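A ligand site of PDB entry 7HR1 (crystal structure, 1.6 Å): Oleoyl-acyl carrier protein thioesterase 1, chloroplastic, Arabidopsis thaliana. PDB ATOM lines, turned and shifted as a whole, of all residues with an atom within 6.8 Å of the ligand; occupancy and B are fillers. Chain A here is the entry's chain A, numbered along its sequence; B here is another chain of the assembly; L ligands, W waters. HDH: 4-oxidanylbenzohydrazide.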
ATOM      1  N   THR A  27      -0.467   5.830 -21.677  1.00  0.00           N
ATOM      2  CA  THR A  27      -1.828   6.364 -21.728  1.00  0.00           C
ATOM      3  C   THR A  27      -2.763   5.376 -20.986  1.00  0.00           C
ATOM      4  O   THR A  27      -2.417   4.180 -20.838  1.00  0.00           O
ATOM      5  CB  THR A  27      -2.308   6.625 -23.174  1.00  0.00           C
ATOM      6  OG1 THR A  27      -2.395   5.375 -23.835  1.00  0.00           O
ATOM      7  CG2 THR A  27      -1.397   7.625 -23.948  1.00  0.00           C
ATOM      8  N   ALA A  28      -3.904   5.865 -20.492  1.00  0.00           N
ATOM      9  CA  ALA A  28      -4.829   5.063 -19.699  1.00  0.00           C
ATOM     10  C   ALA A  28      -5.352   3.861 -20.469  1.00  0.00           C
ATOM     11  O   ALA A  28      -5.639   3.970 -21.669  1.00  0.00           O
ATOM     12  CB  ALA A  28      -5.999   5.921 -19.226  1.00  0.00           C
ATOM     13  N   THR A  29      -5.485   2.709 -19.801  1.00  0.00           N
ATOM     14  CA  THR A  29      -6.031   1.525 -20.446  1.00  0.00           C
ATOM     15  C   THR A  29      -7.556   1.686 -20.581  1.00  0.00           C
ATOM     16  O   THR A  29      -8.154   2.489 -19.852  1.00  0.00           O
ATOM     17  CB  THR A  29      -5.696   0.256 -19.624  1.00  0.00           C
ATOM     18  OG1 THR A  29      -6.435   0.248 -18.399  1.00  0.00           O
ATOM     19  CG2 THR A  29      -4.167   0.106 -19.350  1.00  0.00           C
ATOM     20  N   VAL A  30      -8.207   0.869 -21.427  1.00  0.00           N
ATOM     21  CA  VAL A  30      -9.662   0.872 -21.533  1.00  0.00           C
ATOM     22  C   VAL A  30     -10.316   0.414 -20.210  1.00  0.00           C
ATOM     23  O   VAL A  30     -11.384   0.872 -19.865  1.00  0.00           O
ATOM     24  CB  VAL A  30     -10.147   0.099 -22.773  1.00  0.00           C
ATOM     25  CG1 VAL A  30     -10.097  -1.413 -22.569  1.00  0.00           C
ATOM     26  CG2 VAL A  30     -11.534   0.578 -23.203  1.00  0.00           C
ATOM     27  N   GLU A  31      -9.622  -0.442 -19.426  1.00  0.00           N
ATOM     28  CA  GLU A  31     -10.115  -0.897 -18.124  1.00  0.00           C
ATOM     29  C   GLU A  31     -10.064   0.274 -17.133  1.00  0.00           C
ATOM     30  O   GLU A  31     -11.003   0.427 -16.362  1.00  0.00           O
ATOM     31  CB  GLU A  31      -9.296  -2.098 -17.644  1.00  0.00           C
ATOM     32  CG  GLU A  31      -9.492  -3.282 -18.560  1.00  0.00           C
ATOM     33  CD  GLU A  31      -8.850  -4.545 -18.019  1.00  0.00           C
ATOM     34  OE1 GLU A  31      -7.811  -4.965 -18.588  1.00  0.00           O
ATOM     35  OE2 GLU A  31      -9.388  -5.118 -17.040  1.00  0.00           O
ATOM     36  N   THR A  32      -9.027   1.115 -17.179  1.00  0.00           N
ATOM     37  CA  THR A  32      -8.977   2.329 -16.340  1.00  0.00           C
ATOM     38  C   THR A  32     -10.164   3.248 -16.716  1.00  0.00           C
ATOM     39  O   THR A  32     -10.932   3.649 -15.838  1.00  0.00           O
ATOM     40  CB  THR A  32      -7.623   3.049 -16.447  1.00  0.00           C
ATOM     41  OG1 THR A  32      -6.655   2.310 -15.702  1.00  0.00           O
ATOM     42  CG2 THR A  32      -7.699   4.510 -15.914  1.00  0.00           C
ATOM     43  N   TYR A  80      -6.672   8.107 -25.853  1.00  0.00           N
ATOM     44  CA  TYR A  80      -6.565   7.693 -24.457  1.00  0.00           C
ATOM     45  C   TYR A  80      -5.737   8.774 -23.709  1.00  0.00           C
ATOM     46  O   TYR A  80      -4.653   9.157 -24.189  1.00  0.00           O
ATOM     47  CB  TYR A  80      -5.850   6.331 -24.330  1.00  0.00           C
ATOM     48  CG  TYR A  80      -6.687   5.175 -24.791  1.00  0.00           C
ATOM     49  CD1 TYR A  80      -7.595   4.559 -23.940  1.00  0.00           C
ATOM     50  CD2 TYR A  80      -6.606   4.707 -26.092  1.00  0.00           C
ATOM     51  CE1 TYR A  80      -8.333   3.451 -24.340  1.00  0.00           C
ATOM     52  CE2 TYR A  80      -7.348   3.603 -26.515  1.00  0.00           C
ATOM     53  CZ  TYR A  80      -8.214   2.977 -25.636  1.00  0.00           C
ATOM     54  OH  TYR A  80      -8.984   1.914 -26.056  1.00  0.00           O
ATOM     55  N   ILE A 200     -14.274  -7.170 -19.229  1.00  0.00           N
ATOM     56  CA  ILE A 200     -13.595  -6.474 -20.339  1.00  0.00           C
ATOM     57  C   ILE A 200     -12.122  -6.972 -20.400  1.00  0.00           C
ATOM     58  O   ILE A 200     -11.655  -7.334 -21.468  1.00  0.00           O
ATOM     59  CB  ILE A 200     -13.639  -4.943 -20.133  1.00  0.00           C
ATOM     60  CG1 ILE A 200     -15.098  -4.429 -20.157  1.00  0.00           C
ATOM     61  CG2 ILE A 200     -12.725  -4.221 -21.122  1.00  0.00           C
ATOM     62  CD1 ILE A 200     -15.225  -2.921 -19.825  1.00  0.00           C
ATOM     63  N   GLY A 201     -11.429  -7.020 -19.265  1.00  0.00           N
ATOM     64  CA  GLY A 201     -10.046  -7.508 -19.219  1.00  0.00           C
ATOM     65  C   GLY A 201      -9.932  -8.937 -19.715  1.00  0.00           C
ATOM     66  O   GLY A 201      -9.037  -9.261 -20.515  1.00  0.00           O
ATOM     67  N   VAL A 203     -12.101 -10.545 -21.753  1.00  0.00           N
ATOM     68  CA  VAL A 203     -12.339 -10.564 -23.214  1.00  0.00           C
ATOM     69  C   VAL A 203     -11.027 -10.267 -23.978  1.00  0.00           C
ATOM     70  O   VAL A 203     -10.632 -11.010 -24.895  1.00  0.00           O
ATOM     71  CB  VAL A 203     -13.472  -9.573 -23.639  1.00  0.00           C
ATOM     72  CG1 VAL A 203     -13.410  -9.229 -25.128  1.00  0.00           C
ATOM     73  CG2 VAL A 203     -14.843 -10.133 -23.270  1.00  0.00           C
ATOM     74  N   LEU A 204     -10.344  -9.186 -23.539  1.00  0.00           N
ATOM     75  CA  LEU A 204      -9.143  -8.682 -24.185  1.00  0.00           C
ATOM     76  C   LEU A 204      -7.923  -9.612 -24.015  1.00  0.00           C
ATOM     77  O   LEU A 204      -7.066  -9.609 -24.887  1.00  0.00           O
ATOM     78  CB  LEU A 204      -8.869  -7.243 -23.724  1.00  0.00           C
ATOM     79  CG  LEU A 204      -9.944  -6.229 -24.248  1.00  0.00           C
ATOM     80  CD1 LEU A 204      -9.869  -4.903 -23.538  1.00  0.00           C
ATOM     81  CD2 LEU A 204      -9.849  -6.025 -25.742  1.00  0.00           C
ATOM     82  N   GLU A 205      -7.941 -10.501 -22.995  1.00  0.00           N
ATOM     83  CA  GLU A 205      -6.858 -11.444 -22.773  1.00  0.00           C
ATOM     84  C   GLU A 205      -6.544 -12.338 -23.965  1.00  0.00           C
ATOM     85  O   GLU A 205      -5.383 -12.685 -24.166  1.00  0.00           O
ATOM     86  CB  GLU A 205      -7.099 -12.322 -21.525  1.00  0.00           C
ATOM     87  CG  GLU A 205      -6.614 -11.718 -20.230  1.00  0.00           C
ATOM     88  CD  GLU A 205      -5.130 -11.429 -20.168  1.00  0.00           C
ATOM     89  OE1 GLU A 205      -4.755 -10.243 -20.278  1.00  0.00           O
ATOM     90  OE2 GLU A 205      -4.341 -12.376 -19.946  1.00  0.00           O
ATOM     91  N   SER A 206      -7.569 -12.737 -24.748  1.00  0.00           N
ATOM     92  CA  SER A 206      -7.324 -13.606 -25.911  1.00  0.00           C
ATOM     93  C   SER A 206      -6.937 -12.837 -27.204  1.00  0.00           C
ATOM     94  O   SER A 206      -6.726 -13.487 -28.240  1.00  0.00           O
ATOM     95  CB  SER A 206      -8.497 -14.550 -26.152  1.00  0.00           C
ATOM     96  OG  SER A 206      -9.726 -13.868 -26.236  1.00  0.00           O
ATOM     97  N   ILE A 207      -6.761 -11.520 -27.141  1.00  0.00           N
ATOM     98  CA  ILE A 207      -6.261 -10.761 -28.292  1.00  0.00           C
ATOM     99  C   ILE A 207      -4.734 -10.983 -28.295  1.00  0.00           C
ATOM    100  O   ILE A 207      -4.100 -10.841 -27.239  1.00  0.00           O
ATOM    101  CB  ILE A 207      -6.596  -9.250 -28.149  1.00  0.00           C
ATOM    102  CG1 ILE A 207      -8.102  -8.988 -28.278  1.00  0.00           C
ATOM    103  CG2 ILE A 207      -5.772  -8.388 -29.119  1.00  0.00           C
ATOM    104  CD1 ILE A 207      -8.673  -9.105 -29.753  1.00  0.00           C
ATOM    105  N   VAL A 212      -2.037  -6.010 -29.832  1.00  0.00           N
ATOM    106  CA  VAL A 212      -1.952  -5.042 -28.738  1.00  0.00           C
ATOM    107  C   VAL A 212      -0.758  -4.063 -28.916  1.00  0.00           C
ATOM    108  O   VAL A 212      -0.928  -2.861 -28.783  1.00  0.00           O
ATOM    109  CB  VAL A 212      -1.907  -5.759 -27.365  1.00  0.00           C
ATOM    110  CG1 VAL A 212      -1.786  -4.745 -26.233  1.00  0.00           C
ATOM    111  CG2 VAL A 212      -3.129  -6.635 -27.178  1.00  0.00           C
ATOM    112  N   HIS A 215      -1.497  -1.961 -32.608  1.00  0.00           N
ATOM    113  CA  HIS A 215      -2.799  -1.349 -32.855  1.00  0.00           C
ATOM    114  C   HIS A 215      -3.302  -0.626 -31.644  1.00  0.00           C
ATOM    115  O   HIS A 215      -2.915  -0.944 -30.523  1.00  0.00           O
ATOM    116  CB  HIS A 215      -3.830  -2.435 -33.197  1.00  0.00           C
ATOM    117  CG  HIS A 215      -3.714  -3.033 -34.560  1.00  0.00           C
ATOM    118  ND1 HIS A 215      -2.703  -3.921 -34.874  1.00  0.00           N
ATOM    119  CD2 HIS A 215      -4.550  -2.911 -35.614  1.00  0.00           C
ATOM    120  CE1 HIS A 215      -2.931  -4.288 -36.123  1.00  0.00           C
ATOM    121  NE2 HIS A 215      -4.038  -3.715 -36.614  1.00  0.00           N
ATOM    122  N   GLU A 216      -4.240   0.306 -31.857  1.00  0.00           N
ATOM    123  CA  GLU A 216      -4.920   0.989 -30.784  1.00  0.00           C
ATOM    124  C   GLU A 216      -6.360   0.468 -30.741  1.00  0.00           C
ATOM    125  O   GLU A 216      -6.994   0.376 -31.793  1.00  0.00           O
ATOM    126  CB  GLU A 216      -4.958   2.500 -31.058  1.00  0.00           C
ATOM    127  CG  GLU A 216      -3.637   3.202 -30.804  1.00  0.00           C
ATOM    128  CD  GLU A 216      -3.473   3.673 -29.367  1.00  0.00           C
ATOM    129  OE1 GLU A 216      -2.695   4.631 -29.151  1.00  0.00           O
ATOM    130  OE2 GLU A 216      -4.132   3.119 -28.464  1.00  0.00           O
ATOM    131  N   LEU A 217      -6.886   0.170 -29.563  1.00  0.00           N
ATOM    132  CA  LEU A 217      -8.285  -0.257 -29.423  1.00  0.00           C
ATOM    133  C   LEU A 217      -9.184   0.964 -29.621  1.00  0.00           C
ATOM    134  O   LEU A 217      -9.062   1.947 -28.864  1.00  0.00           O
ATOM    135  CB  LEU A 217      -8.541  -0.859 -28.034  1.00  0.00           C
ATOM    136  CG  LEU A 217      -9.985  -1.246 -27.745  1.00  0.00           C
ATOM    137  CD1 LEU A 217     -10.446  -2.361 -28.685  1.00  0.00           C
ATOM    138  CD2 LEU A 217     -10.147  -1.681 -26.278  1.00  0.00           C
ATOM    139  N   GLN A 218     -10.084   0.918 -30.611  1.00  0.00           N
ATOM    140  CA  GLN A 218     -10.982   2.037 -30.876  1.00  0.00           C
ATOM    141  C   GLN A 218     -12.382   1.844 -30.285  1.00  0.00           C
ATOM    142  O   GLN A 218     -12.933   2.782 -29.719  1.00  0.00           O
ATOM    143  CB  GLN A 218     -11.088   2.341 -32.384  1.00  0.00           C
ATOM    144  CG  GLN A 218      -9.840   2.943 -32.996  1.00  0.00           C
ATOM    145  CD  GLN A 218     -10.222   3.926 -34.086  1.00  0.00           C
ATOM    146  OE1 GLN A 218     -10.300   3.581 -35.270  1.00  0.00           O
ATOM    147  NE2 GLN A 218     -10.504   5.161 -33.679  1.00  0.00           N
ATOM    148  N   TRP A 283     -10.044  -2.268 -33.906  1.00  0.00           N
ATOM    149  CA  TRP A 283      -8.711  -1.762 -33.641  1.00  0.00           C
ATOM    150  C   TRP A 283      -8.180  -1.048 -34.885  1.00  0.00           C
ATOM    151  O   TRP A 283      -8.481  -1.466 -36.007  1.00  0.00           O
ATOM    152  CB  TRP A 283      -7.769  -2.930 -33.325  1.00  0.00           C
ATOM    153  CG  TRP A 283      -8.166  -3.747 -32.127  1.00  0.00           C
ATOM    154  CD1 TRP A 283      -9.234  -4.594 -32.022  1.00  0.00           C
ATOM    155  CD2 TRP A 283      -7.463  -3.823 -30.877  1.00  0.00           C
ATOM    156  NE1 TRP A 283      -9.218  -5.210 -30.782  1.00  0.00           N
ATOM    157  CE2 TRP A 283      -8.171  -4.727 -30.057  1.00  0.00           C
ATOM    158  CE3 TRP A 283      -6.335  -3.172 -30.361  1.00  0.00           C
ATOM    159  CZ2 TRP A 283      -7.783  -4.999 -28.748  1.00  0.00           C
ATOM    160  CZ3 TRP A 283      -5.928  -3.475 -29.073  1.00  0.00           C
ATOM    161  CH2 TRP A 283      -6.643  -4.380 -28.290  1.00  0.00           C
ATOM    162  N   ARG B 184      -2.926 -11.041 -15.594  1.00  0.00           N
ATOM    163  CA  ARG B 184      -3.534 -10.631 -16.853  1.00  0.00           C
ATOM    164  C   ARG B 184      -2.932  -9.216 -17.243  1.00  0.00           C
ATOM    165  O   ARG B 184      -2.171  -8.662 -16.449  1.00  0.00           O
ATOM    166  CB  ARG B 184      -5.078 -10.625 -16.782  1.00  0.00           C
ATOM    167  CG  ARG B 184      -5.711  -9.694 -15.747  1.00  0.00           C
ATOM    168  CD  ARG B 184      -7.206 -10.000 -15.641  1.00  0.00           C
ATOM    169  NE  ARG B 184      -7.877  -9.252 -14.572  1.00  0.00           N
ATOM    170  CZ  ARG B 184      -8.451  -8.057 -14.745  1.00  0.00           C
ATOM    171  NH1 ARG B 184      -8.345  -7.423 -15.907  1.00  0.00           N
ATOM    172  NH2 ARG B 184      -9.106  -7.476 -13.736  1.00  0.00           N
ATOM    173  N   ARG B 185      -3.275  -8.646 -18.426  1.00  0.00           N
ATOM    174  CA  ARG B 185      -2.673  -7.358 -18.830  1.00  0.00           C
ATOM    175  C   ARG B 185      -2.885  -6.233 -17.790  1.00  0.00           C
ATOM    176  O   ARG B 185      -1.963  -5.463 -17.582  1.00  0.00           O
ATOM    177  CB  ARG B 185      -3.080  -6.930 -20.248  1.00  0.00           C
ATOM    178  CG  ARG B 185      -2.524  -7.893 -21.307  1.00  0.00           C
ATOM    179  CD  ARG B 185      -2.451  -7.311 -22.712  1.00  0.00           C
ATOM    180  NE  ARG B 185      -1.939  -8.310 -23.631  1.00  0.00           N
ATOM    181  CZ  ARG B 185      -2.683  -9.040 -24.445  1.00  0.00           C
ATOM    182  NH1 ARG B 185      -3.996  -8.843 -24.520  1.00  0.00           N
ATOM    183  NH2 ARG B 185      -2.119  -9.950 -25.237  1.00  0.00           N
ATOM    184  N   ALA B 186      -4.022  -6.200 -17.087  1.00  0.00           N
ATOM    185  CA  ALA B 186      -4.252  -5.190 -16.054  1.00  0.00           C
ATOM    186  C   ALA B 186      -3.279  -5.289 -14.866  1.00  0.00           C
ATOM    187  O   ALA B 186      -3.046  -4.286 -14.206  1.00  0.00           O
ATOM    188  CB  ALA B 186      -5.703  -5.214 -15.581  1.00  0.00           C
HETATM  189  C1  HDH L   1      -5.753  -5.805 -23.067  1.00  0.00           C
HETATM  190  C2  HDH L   1      -5.461  -5.269 -24.314  1.00  0.00           C
HETATM  191  C3  HDH L   1      -5.615  -3.906 -24.541  1.00  0.00           C
HETATM  192  C8  HDH L   1      -6.174  -1.585 -23.648  1.00  0.00           C
HETATM  193  C4  HDH L   1      -6.063  -3.064 -23.518  1.00  0.00           C
HETATM  194  C5  HDH L   1      -6.382  -3.624 -22.274  1.00  0.00           C
HETATM  195  C6  HDH L   1      -6.224  -4.978 -22.051  1.00  0.00           C
HETATM  196  O7  HDH L   1      -5.607  -7.134 -22.830  1.00  0.00           O
HETATM  197  O10 HDH L   1      -6.495  -0.896 -22.682  1.00  0.00           O
HETATM  198  N9  HDH L   1      -5.944  -1.056 -24.847  1.00  0.00           N
HETATM  199  N17 HDH L   1      -6.322   0.277 -25.134  1.00  0.00           N
HETATM  200  O   HOH W   1      -6.524  -8.225 -20.585  1.00  0.00           O
HETATM  201  O   HOH W   2      -5.089   0.718 -27.349  1.00  0.00           O
HETATM  202  O   HOH W   3      -3.376  -1.656 -27.061  1.00  0.00           O
HETATM  203  O   HOH W   4      -4.325   2.483 -23.680  1.00  0.00           O
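The guanidinium group (NH1) of Arg 185 of chain B sits at hydrogen-bond distance from an oxygen (O7) of the ligand (2.9 Å). A nitrogen (N17) of the ligand is in hydrogen-bond range of the side-chain hydroxyl (OH) of Tyr 80 (3.3 Å). N of Val 30 sits at hydrogen-bond distance from O10 of the ligand (2.8 Å).
The backbone carbonyl oxygen (O) of Ile 207 sits at hydrogen-bond distance from the guanidinium group (NH2) of Arg 185 of chain B, at 3.0 Å. The backbone NH (N) of Arg 185 of chain B is in hydrogen-bond range of the side-chain carboxylate (OE1) of Glu 205 (2.9 Å). The side-chain carboxylate (OE2) of Glu 31 lies within salt-bridge range of the guanidinium group (NH1) of Arg 184 of chain B (2.8 Å). The side-chain hydroxyl of Thr 29 lies close to the backbone NH of Glu 31 (3.4 Å). The guanidinium group (NH1) of Arg 185 of chain B lies within hydrogen-bond range of the backbone carbonyl oxygen (O) of Leu 204 (3.2 Å). OG1 of Thr 29 is in hydrogen-bond range of N of Thr 32, at 3.0 Å. The side-chain hydroxyl of Tyr 80 lies within hydrogen-bond range of the backbone carbonyl oxygen of Leu 217, at 2.8 Å.
Merely in contact with the ligand: Thr 29 (3.3 Å), Glu 31 (3.8 Å), Leu 204 (3.4 Å), Val 212 (3.9 Å), Leu 217 (3.8 Å) and Trp 283 (3.9 Å). Of the 23 residues printed, 9 come within 4 Å of the ligand.
Water W2 lies within hydrogen-bond range of a nitrogen (N17) of the ligand (2.6 Å), the side-chain carboxylate (OE2) of Glu 216 (2.8 Å) and the backbone NH (N) of Leu 217 (2.9 Å). Water W1 lies within hydrogen-bond range of an oxygen (O7) of the ligand (2.7 Å), the side-chain carboxylate of Glu 205 (2.7 Å) and the backbone carbonyl oxygen of Gly 201 (2.7 Å). Water W4 lies within hydrogen-bond range of O of Ala 28, N17 of the ligand and OG1 of Thr 27. Water W3 bridges O of Val 212 and N9 of the ligand.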
